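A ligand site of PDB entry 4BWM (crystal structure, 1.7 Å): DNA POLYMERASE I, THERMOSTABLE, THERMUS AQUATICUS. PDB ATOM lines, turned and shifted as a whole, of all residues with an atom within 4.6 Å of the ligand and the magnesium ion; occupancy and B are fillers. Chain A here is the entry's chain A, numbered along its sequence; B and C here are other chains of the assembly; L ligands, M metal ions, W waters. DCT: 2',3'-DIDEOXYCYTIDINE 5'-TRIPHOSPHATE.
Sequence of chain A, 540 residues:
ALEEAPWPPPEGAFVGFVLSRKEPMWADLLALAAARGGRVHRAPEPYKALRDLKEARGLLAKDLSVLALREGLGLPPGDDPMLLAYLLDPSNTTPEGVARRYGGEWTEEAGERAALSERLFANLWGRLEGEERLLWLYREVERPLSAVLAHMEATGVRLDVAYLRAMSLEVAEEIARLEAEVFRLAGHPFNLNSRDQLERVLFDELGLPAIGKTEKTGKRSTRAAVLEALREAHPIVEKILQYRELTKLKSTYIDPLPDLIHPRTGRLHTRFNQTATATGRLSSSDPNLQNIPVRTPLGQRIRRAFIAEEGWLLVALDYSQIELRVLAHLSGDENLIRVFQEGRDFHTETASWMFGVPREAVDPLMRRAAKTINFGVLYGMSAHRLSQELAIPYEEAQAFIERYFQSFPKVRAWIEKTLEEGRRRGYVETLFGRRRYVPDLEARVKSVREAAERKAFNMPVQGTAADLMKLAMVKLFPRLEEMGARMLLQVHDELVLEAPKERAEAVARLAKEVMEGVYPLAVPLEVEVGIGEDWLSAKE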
ATOM      1  N   ASP A 318      13.243 -39.007   3.185  1.00  0.00           N
ATOM      2  CA  ASP A 318      13.360 -37.716   2.478  1.00  0.00           C
ATOM      3  C   ASP A 318      12.974 -36.575   3.405  1.00  0.00           C
ATOM      4  O   ASP A 318      11.884 -36.587   3.961  1.00  0.00           O
ATOM      5  CB  ASP A 318      12.426 -37.720   1.250  1.00  0.00           C
ATOM      6  CG  ASP A 318      12.732 -36.598   0.263  1.00  0.00           C
ATOM      7  OD1 ASP A 318      13.878 -36.129   0.204  1.00  0.00           O
ATOM      8  OD2 ASP A 318      11.806 -36.201  -0.485  1.00  0.00           O
ATOM      9  N   TYR A 319      13.843 -35.569   3.549  1.00  0.00           N
ATOM     10  CA  TYR A 319      13.447 -34.401   4.313  1.00  0.00           C
ATOM     11  C   TYR A 319      12.412 -33.609   3.516  1.00  0.00           C
ATOM     12  O   TYR A 319      12.669 -33.211   2.379  1.00  0.00           O
ATOM     13  CB  TYR A 319      14.648 -33.489   4.616  1.00  0.00           C
ATOM     14  CG  TYR A 319      15.453 -33.823   5.856  1.00  0.00           C
ATOM     15  CD1 TYR A 319      14.937 -33.635   7.134  1.00  0.00           C
ATOM     16  CD2 TYR A 319      16.763 -34.259   5.736  1.00  0.00           C
ATOM     17  CE1 TYR A 319      15.708 -33.912   8.274  1.00  0.00           C
ATOM     18  CE2 TYR A 319      17.530 -34.543   6.853  1.00  0.00           C
ATOM     19  CZ  TYR A 319      17.011 -34.363   8.108  1.00  0.00           C
ATOM     20  OH  TYR A 319      17.788 -34.646   9.196  1.00  0.00           O
ATOM     21  N   GLN A 321      10.657 -30.530   2.281  1.00  0.00           N
ATOM     22  CA  GLN A 321      10.816 -29.076   2.165  1.00  0.00           C
ATOM     23  C   GLN A 321      11.811 -28.479   3.167  1.00  0.00           C
ATOM     24  O   GLN A 321      11.569 -27.411   3.754  1.00  0.00           O
ATOM     25  CB  GLN A 321       9.442 -28.383   2.267  1.00  0.00           C
ATOM     26  CG  GLN A 321       8.593 -28.715   1.070  1.00  0.00           C
ATOM     27  CD  GLN A 321       7.105 -28.428   1.231  1.00  0.00           C
ATOM     28  OE1 GLN A 321       6.668 -27.695   2.127  1.00  0.00           O
ATOM     29  NE2 GLN A 321       6.304 -29.017   0.332  1.00  0.00           N
ATOM     30  N   GLU A 323      14.733 -26.957   2.858  1.00  0.00           N
ATOM     31  CA  GLU A 323      15.258 -25.614   2.604  1.00  0.00           C
ATOM     32  C   GLU A 323      14.280 -24.505   2.991  1.00  0.00           C
ATOM     33  O   GLU A 323      14.687 -23.474   3.530  1.00  0.00           O
ATOM     34  CB  GLU A 323      15.718 -25.432   1.165  1.00  0.00           C
ATOM     35  CG  GLU A 323      17.014 -26.132   0.847  1.00  0.00           C
ATOM     36  CD  GLU A 323      17.648 -25.607  -0.422  1.00  0.00           C
ATOM     37  OE1 GLU A 323      17.456 -24.412  -0.726  1.00  0.00           O
ATOM     38  OE2 GLU A 323      18.322 -26.401  -1.111  1.00  0.00           O
ATOM     39  N   LEU A 324      12.988 -24.719   2.733  1.00  0.00           N
ATOM     40  CA  LEU A 324      11.963 -23.751   3.143  1.00  0.00           C
ATOM     41  C   LEU A 324      11.834 -23.678   4.662  1.00  0.00           C
ATOM     42  O   LEU A 324      11.610 -22.604   5.227  1.00  0.00           O
ATOM     43  CB  LEU A 324      10.616 -24.065   2.496  1.00  0.00           C
ATOM     44  CG  LEU A 324      10.566 -23.840   0.984  1.00  0.00           C
ATOM     45  CD1 LEU A 324       9.425 -24.620   0.355  1.00  0.00           C
ATOM     46  CD2 LEU A 324      10.461 -22.342   0.671  1.00  0.00           C
ATOM     47  N   HIS A 347       4.096 -25.427  -1.086  1.00  0.00           N
ATOM     48  CA  HIS A 347       3.901 -25.230  -2.515  1.00  0.00           C
ATOM     49  C   HIS A 347       2.424 -25.315  -2.875  1.00  0.00           C
ATOM     50  O   HIS A 347       1.974 -24.678  -3.821  1.00  0.00           O
ATOM     51  CB  HIS A 347       4.717 -26.232  -3.321  1.00  0.00           C
ATOM     52  CG  HIS A 347       6.196 -26.109  -3.112  1.00  0.00           C
ATOM     53  ND1 HIS A 347       6.911 -24.987  -3.453  1.00  0.00           N
ATOM     54  CD2 HIS A 347       7.091 -26.984  -2.601  1.00  0.00           C
ATOM     55  CE1 HIS A 347       8.176 -25.165  -3.148  1.00  0.00           C
ATOM     56  NE2 HIS A 347       8.321 -26.373  -2.637  1.00  0.00           N
ATOM     57  N   ARG A 367       0.993 -27.650  -9.056  1.00  0.00           N
ATOM     58  CA  ARG A 367       1.963 -27.609  -7.964  1.00  0.00           C
ATOM     59  C   ARG A 367       3.392 -27.458  -8.477  1.00  0.00           C
ATOM     60  O   ARG A 367       4.200 -26.719  -7.902  1.00  0.00           O
ATOM     61  CB  ARG A 367       1.845 -28.842  -7.076  1.00  0.00           C
ATOM     62  CG  ARG A 367       2.645 -28.746  -5.768  1.00  0.00           C
ATOM     63  CD  ARG A 367       2.387 -29.950  -4.869  1.00  0.00           C
ATOM     64  NE  ARG A 367       3.097 -29.853  -3.592  1.00  0.00           N
ATOM     65  CZ  ARG A 367       4.374 -30.185  -3.424  1.00  0.00           C
ATOM     66  NH1 ARG A 367       5.086 -30.609  -4.449  1.00  0.00           N
ATOM     67  NH2 ARG A 367       4.942 -30.071  -2.222  1.00  0.00           N
ATOM     68  N   LYS A 371       5.919 -24.369  -7.767  1.00  0.00           N
ATOM     69  CA  LYS A 371       7.243 -24.574  -7.179  1.00  0.00           C
ATOM     70  C   LYS A 371       8.307 -23.791  -7.920  1.00  0.00           C
ATOM     71  O   LYS A 371       9.186 -23.177  -7.302  1.00  0.00           O
ATOM     72  CB  LYS A 371       7.641 -26.052  -7.204  1.00  0.00           C
ATOM     73  CG  LYS A 371       6.908 -26.914  -6.200  1.00  0.00           C
ATOM     74  CD  LYS A 371       7.370 -28.364  -6.295  1.00  0.00           C
ATOM     75  CE  LYS A 371       8.869 -28.522  -6.035  1.00  0.00           C
ATOM     76  NZ  LYS A 371       9.315 -29.956  -6.128  1.00  0.00           N
ATOM     77  N   PHE A 375      10.567 -20.852  -6.054  1.00  0.00           N
ATOM     78  CA  PHE A 375      12.017 -20.871  -5.954  1.00  0.00           C
ATOM     79  C   PHE A 375      12.639 -19.698  -6.714  1.00  0.00           C
ATOM     80  O   PHE A 375      13.551 -19.044  -6.214  1.00  0.00           O
ATOM     81  CB  PHE A 375      12.575 -22.196  -6.486  1.00  0.00           C
ATOM     82  CG  PHE A 375      12.158 -23.401  -5.681  1.00  0.00           C
ATOM     83  CD1 PHE A 375      12.029 -23.345  -4.313  1.00  0.00           C
ATOM     84  CD2 PHE A 375      11.874 -24.598  -6.321  1.00  0.00           C
ATOM     85  CE1 PHE A 375      11.650 -24.471  -3.583  1.00  0.00           C
ATOM     86  CE2 PHE A 375      11.509 -25.715  -5.596  1.00  0.00           C
ATOM     87  CZ  PHE A 375      11.378 -25.642  -4.225  1.00  0.00           C
ATOM     88  N   TYR A 379      14.304 -16.730  -4.378  1.00  0.00           N
ATOM     89  CA  TYR A 379      15.760 -16.738  -4.444  1.00  0.00           C
ATOM     90  C   TYR A 379      16.371 -15.812  -5.486  1.00  0.00           C
ATOM     91  O   TYR A 379      17.555 -15.933  -5.800  1.00  0.00           O
ATOM     92  CB  TYR A 379      16.283 -18.180  -4.572  1.00  0.00           C
ATOM     93  CG  TYR A 379      15.789 -19.085  -3.446  1.00  0.00           C
ATOM     94  CD1 TYR A 379      15.935 -18.699  -2.110  1.00  0.00           C
ATOM     95  CD2 TYR A 379      15.148 -20.294  -3.713  1.00  0.00           C
ATOM     96  CE1 TYR A 379      15.479 -19.511  -1.073  1.00  0.00           C
ATOM     97  CE2 TYR A 379      14.684 -21.102  -2.671  1.00  0.00           C
ATOM     98  CZ  TYR A 379      14.853 -20.704  -1.351  1.00  0.00           C
ATOM     99  OH  TYR A 379      14.403 -21.496  -0.321  1.00  0.00           O
ATOM    100  N   GLN A 462      20.720 -22.975   1.477  1.00  0.00           N
ATOM    101  CA  GLN A 462      21.144 -24.255   0.902  1.00  0.00           C
ATOM    102  C   GLN A 462      22.207 -24.939   1.742  1.00  0.00           C
ATOM    103  O   GLN A 462      22.147 -26.153   1.960  1.00  0.00           O
ATOM    104  CB  GLN A 462      21.676 -24.083  -0.531  1.00  0.00           C
ATOM    105  CG  GLN A 462      20.720 -23.441  -1.503  1.00  0.00           C
ATOM    106  CD  GLN A 462      21.307 -23.365  -2.904  1.00  0.00           C
ATOM    107  OE1 GLN A 462      22.462 -22.977  -3.081  1.00  0.00           O
ATOM    108  NE2 GLN A 462      20.512 -23.726  -3.895  1.00  0.00           N
ATOM    109  N   ASP A 493      17.511 -34.317  -1.022  1.00  0.00           N
ATOM    110  CA  ASP A 493      17.246 -34.230   0.434  1.00  0.00           C
ATOM    111  C   ASP A 493      16.954 -35.625   1.023  1.00  0.00           C
ATOM    112  O   ASP A 493      16.338 -35.762   2.093  1.00  0.00           O
ATOM    113  CB  ASP A 493      16.015 -33.347   0.673  1.00  0.00           C
ATOM    114  CG  ASP A 493      16.234 -31.893   0.219  1.00  0.00           C
ATOM    115  OD1 ASP A 493      17.392 -31.425   0.232  1.00  0.00           O
ATOM    116  OD2 ASP A 493      15.246 -31.231  -0.143  1.00  0.00           O
ATOM    117  P     G B   4      16.896 -13.812 -13.738  1.00  0.00           P
ATOM    118  OP1   G B   4      16.295 -15.115 -14.076  1.00  0.00           O
ATOM    119  OP2   G B   4      16.028 -12.617 -13.534  1.00  0.00           O
ATOM    120  O5'   G B   4      17.728 -14.020 -12.404  1.00  0.00           O
ATOM    121  C5'   G B   4      18.407 -15.239 -12.139  1.00  0.00           C
ATOM    122  C4'   G B   4      18.486 -15.495 -10.660  1.00  0.00           C
ATOM    123  O4'   G B   4      17.183 -15.888 -10.169  1.00  0.00           O
ATOM    124  C3'   G B   4      19.422 -16.615 -10.235  1.00  0.00           C
ATOM    125  O3'   G B   4      20.748 -16.151 -10.133  1.00  0.00           O
ATOM    126  C2'   G B   4      18.820 -17.041  -8.903  1.00  0.00           C
ATOM    127  O2'   G B   4      19.179 -16.109  -7.883  1.00  0.00           O
ATOM    128  C1'   G B   4      17.332 -16.889  -9.184  1.00  0.00           C
ATOM    129  N9    G B   4      16.712 -18.122  -9.698  1.00  0.00           N
ATOM    130  C8    G B   4      16.098 -18.255 -10.922  1.00  0.00           C
ATOM    131  N7    G B   4      15.603 -19.450 -11.111  1.00  0.00           N
ATOM    132  C5    G B   4      15.883 -20.126  -9.932  1.00  0.00           C
ATOM    133  C6    G B   4      15.584 -21.467  -9.550  1.00  0.00           C
ATOM    134  O6    G B   4      14.984 -22.325 -10.203  1.00  0.00           O
ATOM    135  N1    G B   4      16.073 -21.751  -8.280  1.00  0.00           N
ATOM    136  C2    G B   4      16.737 -20.889  -7.459  1.00  0.00           C
ATOM    137  N2    G B   4      17.111 -21.373  -6.262  1.00  0.00           N
ATOM    138  N3    G B   4      17.024 -19.634  -7.802  1.00  0.00           N
ATOM    139  C4    G B   4      16.565 -19.324  -9.042  1.00  0.00           C
ATOM    140  P     G B   5      22.003 -17.103 -10.401  1.00  0.00           P
ATOM    141  OP1   G B   5      23.166 -16.183 -10.416  1.00  0.00           O
ATOM    142  OP2   G B   5      21.715 -17.960 -11.573  1.00  0.00           O
ATOM    143  O5'   G B   5      22.057 -18.041  -9.115  1.00  0.00           O
ATOM    144  C5'   G B   5      22.360 -17.520  -7.821  1.00  0.00           C
ATOM    145  C4'   G B   5      22.378 -18.622  -6.802  1.00  0.00           C
ATOM    146  O4'   G B   5      21.039 -19.151  -6.650  1.00  0.00           O
ATOM    147  C3'   G B   5      23.224 -19.838  -7.147  1.00  0.00           C
ATOM    148  O3'   G B   5      24.593 -19.673  -6.836  1.00  0.00           O
ATOM    149  C2'   G B   5      22.555 -20.947  -6.349  1.00  0.00           C
ATOM    150  O2'   G B   5      22.922 -20.852  -4.968  1.00  0.00           O
ATOM    151  C1'   G B   5      21.088 -20.552  -6.470  1.00  0.00           C
ATOM    152  N9    G B   5      20.418 -21.180  -7.627  1.00  0.00           N
ATOM    153  C8    G B   5      20.096 -20.579  -8.814  1.00  0.00           C
ATOM    154  N7    G B   5      19.477 -21.361  -9.650  1.00  0.00           N
ATOM    155  C5    G B   5      19.369 -22.563  -8.965  1.00  0.00           C
ATOM    156  C6    G B   5      18.782 -23.789  -9.352  1.00  0.00           C
ATOM    157  O6    G B   5      18.211 -24.073 -10.415  1.00  0.00           O
ATOM    158  N1    G B   5      18.905 -24.754  -8.358  1.00  0.00           N
ATOM    159  C2    G B   5      19.499 -24.557  -7.139  1.00  0.00           C
ATOM    160  N2    G B   5      19.488 -25.617  -6.312  1.00  0.00           N
ATOM    161  N3    G B   5      20.052 -23.418  -6.759  1.00  0.00           N
ATOM    162  C4    G B   5      19.940 -22.471  -7.713  1.00  0.00           C
ATOM    163  N1  DOC C  12      16.927 -29.505  -8.330  1.00  0.00           N
ATOM    164  C2  DOC C  12      17.534 -28.311  -8.066  1.00  0.00           C
ATOM    165  N3  DOC C  12      17.415 -27.251  -8.883  1.00  0.00           N
ATOM    166  C4  DOC C  12      16.676 -27.342 -10.006  1.00  0.00           C
ATOM    167  C5  DOC C  12      16.036 -28.531 -10.340  1.00  0.00           C
ATOM    168  C6  DOC C  12      16.185 -29.640  -9.442  1.00  0.00           C
ATOM    169  O2  DOC C  12      18.210 -28.151  -7.060  1.00  0.00           O
ATOM    170  N4  DOC C  12      16.546 -26.195 -10.907  1.00  0.00           N
ATOM    171  C1' DOC C  12      17.027 -30.647  -7.470  1.00  0.00           C
ATOM    172  C2' DOC C  12      15.931 -30.700  -6.456  1.00  0.00           C
ATOM    173  C3' DOC C  12      15.011 -31.700  -6.920  1.00  0.00           C
ATOM    174  C4' DOC C  12      15.863 -32.645  -7.664  1.00  0.00           C
ATOM    175  O4' DOC C  12      16.947 -31.866  -8.172  1.00  0.00           O
ATOM    176  C5' DOC C  12      15.118 -33.309  -8.715  1.00  0.00           C
ATOM    177  O5' DOC C  12      14.424 -32.497  -9.613  1.00  0.00           O
ATOM    178  P   DOC C  12      13.970 -33.116 -11.004  1.00  0.00           P
ATOM    179  OP1 DOC C  12      12.994 -34.284 -10.766  1.00  0.00           O
ATOM    180  OP2 DOC C  12      13.312 -31.994 -11.801  1.00  0.00           O
HETATM  181  N1  DCT L   1      15.534 -26.032  -5.693  1.00  0.00           N
HETATM  182  C2  DCT L   1      15.802 -24.778  -6.215  1.00  0.00           C
HETATM  183  N3  DCT L   1      15.286 -24.432  -7.433  1.00  0.00           N
HETATM  184  C4  DCT L   1      14.501 -25.300  -8.146  1.00  0.00           C
HETATM  185  C5  DCT L   1      14.213 -26.568  -7.626  1.00  0.00           C
HETATM  186  C6  DCT L   1      14.746 -26.913  -6.376  1.00  0.00           C
HETATM  187  O2  DCT L   1      16.512 -23.998  -5.583  1.00  0.00           O
HETATM  188  N4  DCT L   1      14.026 -24.923  -9.315  1.00  0.00           N
HETATM  189  C1' DCT L   1      16.079 -26.364  -4.385  1.00  0.00           C
HETATM  190  C2' DCT L   1      15.103 -25.821  -3.342  1.00  0.00           C
HETATM  191  C3' DCT L   1      14.528 -27.043  -2.634  1.00  0.00           C
HETATM  192  C4' DCT L   1      15.498 -28.155  -3.011  1.00  0.00           C
HETATM  193  O4' DCT L   1      16.063 -27.776  -4.248  1.00  0.00           O
HETATM  194  C5' DCT L   1      14.768 -29.499  -3.103  1.00  0.00           C
HETATM  195  O5' DCT L   1      13.860 -29.545  -4.168  1.00  0.00           O
HETATM  196  PA  DCT L   1      12.438 -30.255  -4.024  1.00  0.00           P
HETATM  197  O1A DCT L   1      11.801 -30.509  -5.365  1.00  0.00           O
HETATM  198  O2A DCT L   1      12.553 -31.464  -3.118  1.00  0.00           O
HETATM  199  O3A DCT L   1      11.588 -29.049  -3.365  1.00  0.00           O
HETATM  200  PB  DCT L   1      10.688 -29.099  -2.048  1.00  0.00           P
HETATM  201  O1B DCT L   1      11.248 -30.050  -1.011  1.00  0.00           O
HETATM  202  O2B DCT L   1      10.585 -27.706  -1.488  1.00  0.00           O
HETATM  203  O3B DCT L   1       9.240 -29.471  -2.644  1.00  0.00           O
HETATM  204  PG  DCT L   1       8.626 -30.970  -2.694  1.00  0.00           P
HETATM  205  O1G DCT L   1       9.745 -31.950  -2.672  1.00  0.00           O
HETATM  206  O2G DCT L   1       7.752 -31.088  -3.910  1.00  0.00           O
HETATM  207  O3G DCT L   1       7.805 -31.149  -1.454  1.00  0.00           O
HETATM  208 MG    MG M   1      11.372 -32.037  -1.639  1.00  0.00          MG
HETATM  209  O   HOH W   1      12.755 -32.130  -0.281  1.00  0.00           O
HETATM  210  O   HOH W   2      10.102 -32.628  -0.123  1.00  0.00           O
HETATM  211  O   HOH W   3       8.581 -34.986  -2.516  1.00  0.00           O
HETATM  212  O   HOH W   4      11.498 -33.153  -6.364  1.00  0.00           O
HETATM  213  O   HOH W   5      11.503 -34.070  -2.183  1.00  0.00           O
HETATM  214  O   HOH W   6      18.454 -29.265  -4.707  1.00  0.00           O
HETATM  215  O   HOH W   7      12.398 -26.716   0.304  1.00  0.00           O
HETATM  216  O   HOH W   8      17.194 -31.500  -3.039  1.00  0.00           O
HETATM  217  O   HOH W   9      14.839 -32.905  -3.204  1.00  0.00           O
HETATM  218  O   HOH W  10      12.400 -29.286  -7.987  1.00  0.00           O
HETATM  219  O   HOH W  11      13.559 -23.996  -1.123  1.00  0.00           O
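The guanidinium group (NH2) of Arg 367 sits close to the side-chain amide nitrogen (NE2) of Gln 321, 3.1 Å away.
O2' of G 4 of chain B lies close to the backbone carbonyl oxygen (O) of Tyr 379.
N4 of DOC 12 of chain C lies close to O6 of G 5 of chain B, 2.7 Å away.
O2' of G 5 of chain B sits close to the side-chain amide oxygen (OE1) of Gln 462 (2.9 Å).
The backbone carbonyl oxygen (O) of Asp 493 sits at hydrogen-bond distance from the backbone NH (N) of Tyr 319 (2.9 Å).
An oxygen (O1A) of the ligand is in salt-bridge range of the side-chain amino group of Lys 371 (2.7 Å).
O2G of the ligand lies within salt-bridge range of NH1 of Arg 367 (2.8 Å).
N4 of the ligand is in hydrogen-bond range of O6 of G 4 of chain B, at 2.9 Å.
An oxygen (O2B) of the ligand lies within hydrogen-bond range of a ring nitrogen (NE2) of His 347 (2.9 Å).
The backbone NH of Gln 321 lies close to an oxygen (O1B) of the ligand (3.4 Å).
An oxygen (O3G) of the ligand sits at hydrogen-bond distance from the side-chain amide nitrogen (NE2) of Gln 321, 3.2 Å away.
N4 of DOC 12 of chain C lies within hydrogen-bond range of a nitrogen (N4) of the ligand, 3.2 Å away.
The magnesium ion is bound by O1G of the ligand, water W1, O2A of the ligand, water W2, O1B of the ligand and water W5.
The magnesium ion has six donor atoms within binding distance.
Water W1 bridges the side-chain carboxylate of Asp 493 (2.7 Å) and the backbone carbonyl oxygen of Tyr 319 (2.9 Å).
Water W2 bridges O3G of the ligand (3.0 Å) and N of Gln 321 (3.2 Å).
Water W7 lies within hydrogen-bond range of an oxygen (O2B) of the ligand (2.7 Å), the backbone NH (N) of Leu 324 (3.2 Å) and the backbone NH (N) of Glu 323 (3.5 Å).
Water W6 lies within hydrogen-bond range of O2 of DOC 12 of chain C (2.6 Å) and O4' of the ligand (2.9 Å).
N2 of G 5 of chain B sits close to O2 of the ligand (3.5 Å).
Residues that only touch the ligand: Glu 323 (3.8 Å), Leu 324 (3.8 Å), Phe 375 (3.3 Å) and Asp 493 (3.5 Å).
Hydrophobic or aromatic side chains that line the ligand: Leu 324, His 347 and Phe 375.
Within 4 Å of the ligand: Gln 321, Glu 323, Leu 324, His 347, Arg 367, Lys 371, Phe 375, Asp 493, G 4 of chain B, G 5 of chain B and DOC 12 of chain C.
Along chain A the residues within 4 Å of the ligand span positions 321 to 493.
The nearest printed residue that does not touch the ligand is Gln 462 (4.4 Å).
No residue comes within 4 Å of the magnesium ion.
The nearest printed residue that does not touch the magnesium ion is Asp 493 (4.2 Å).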
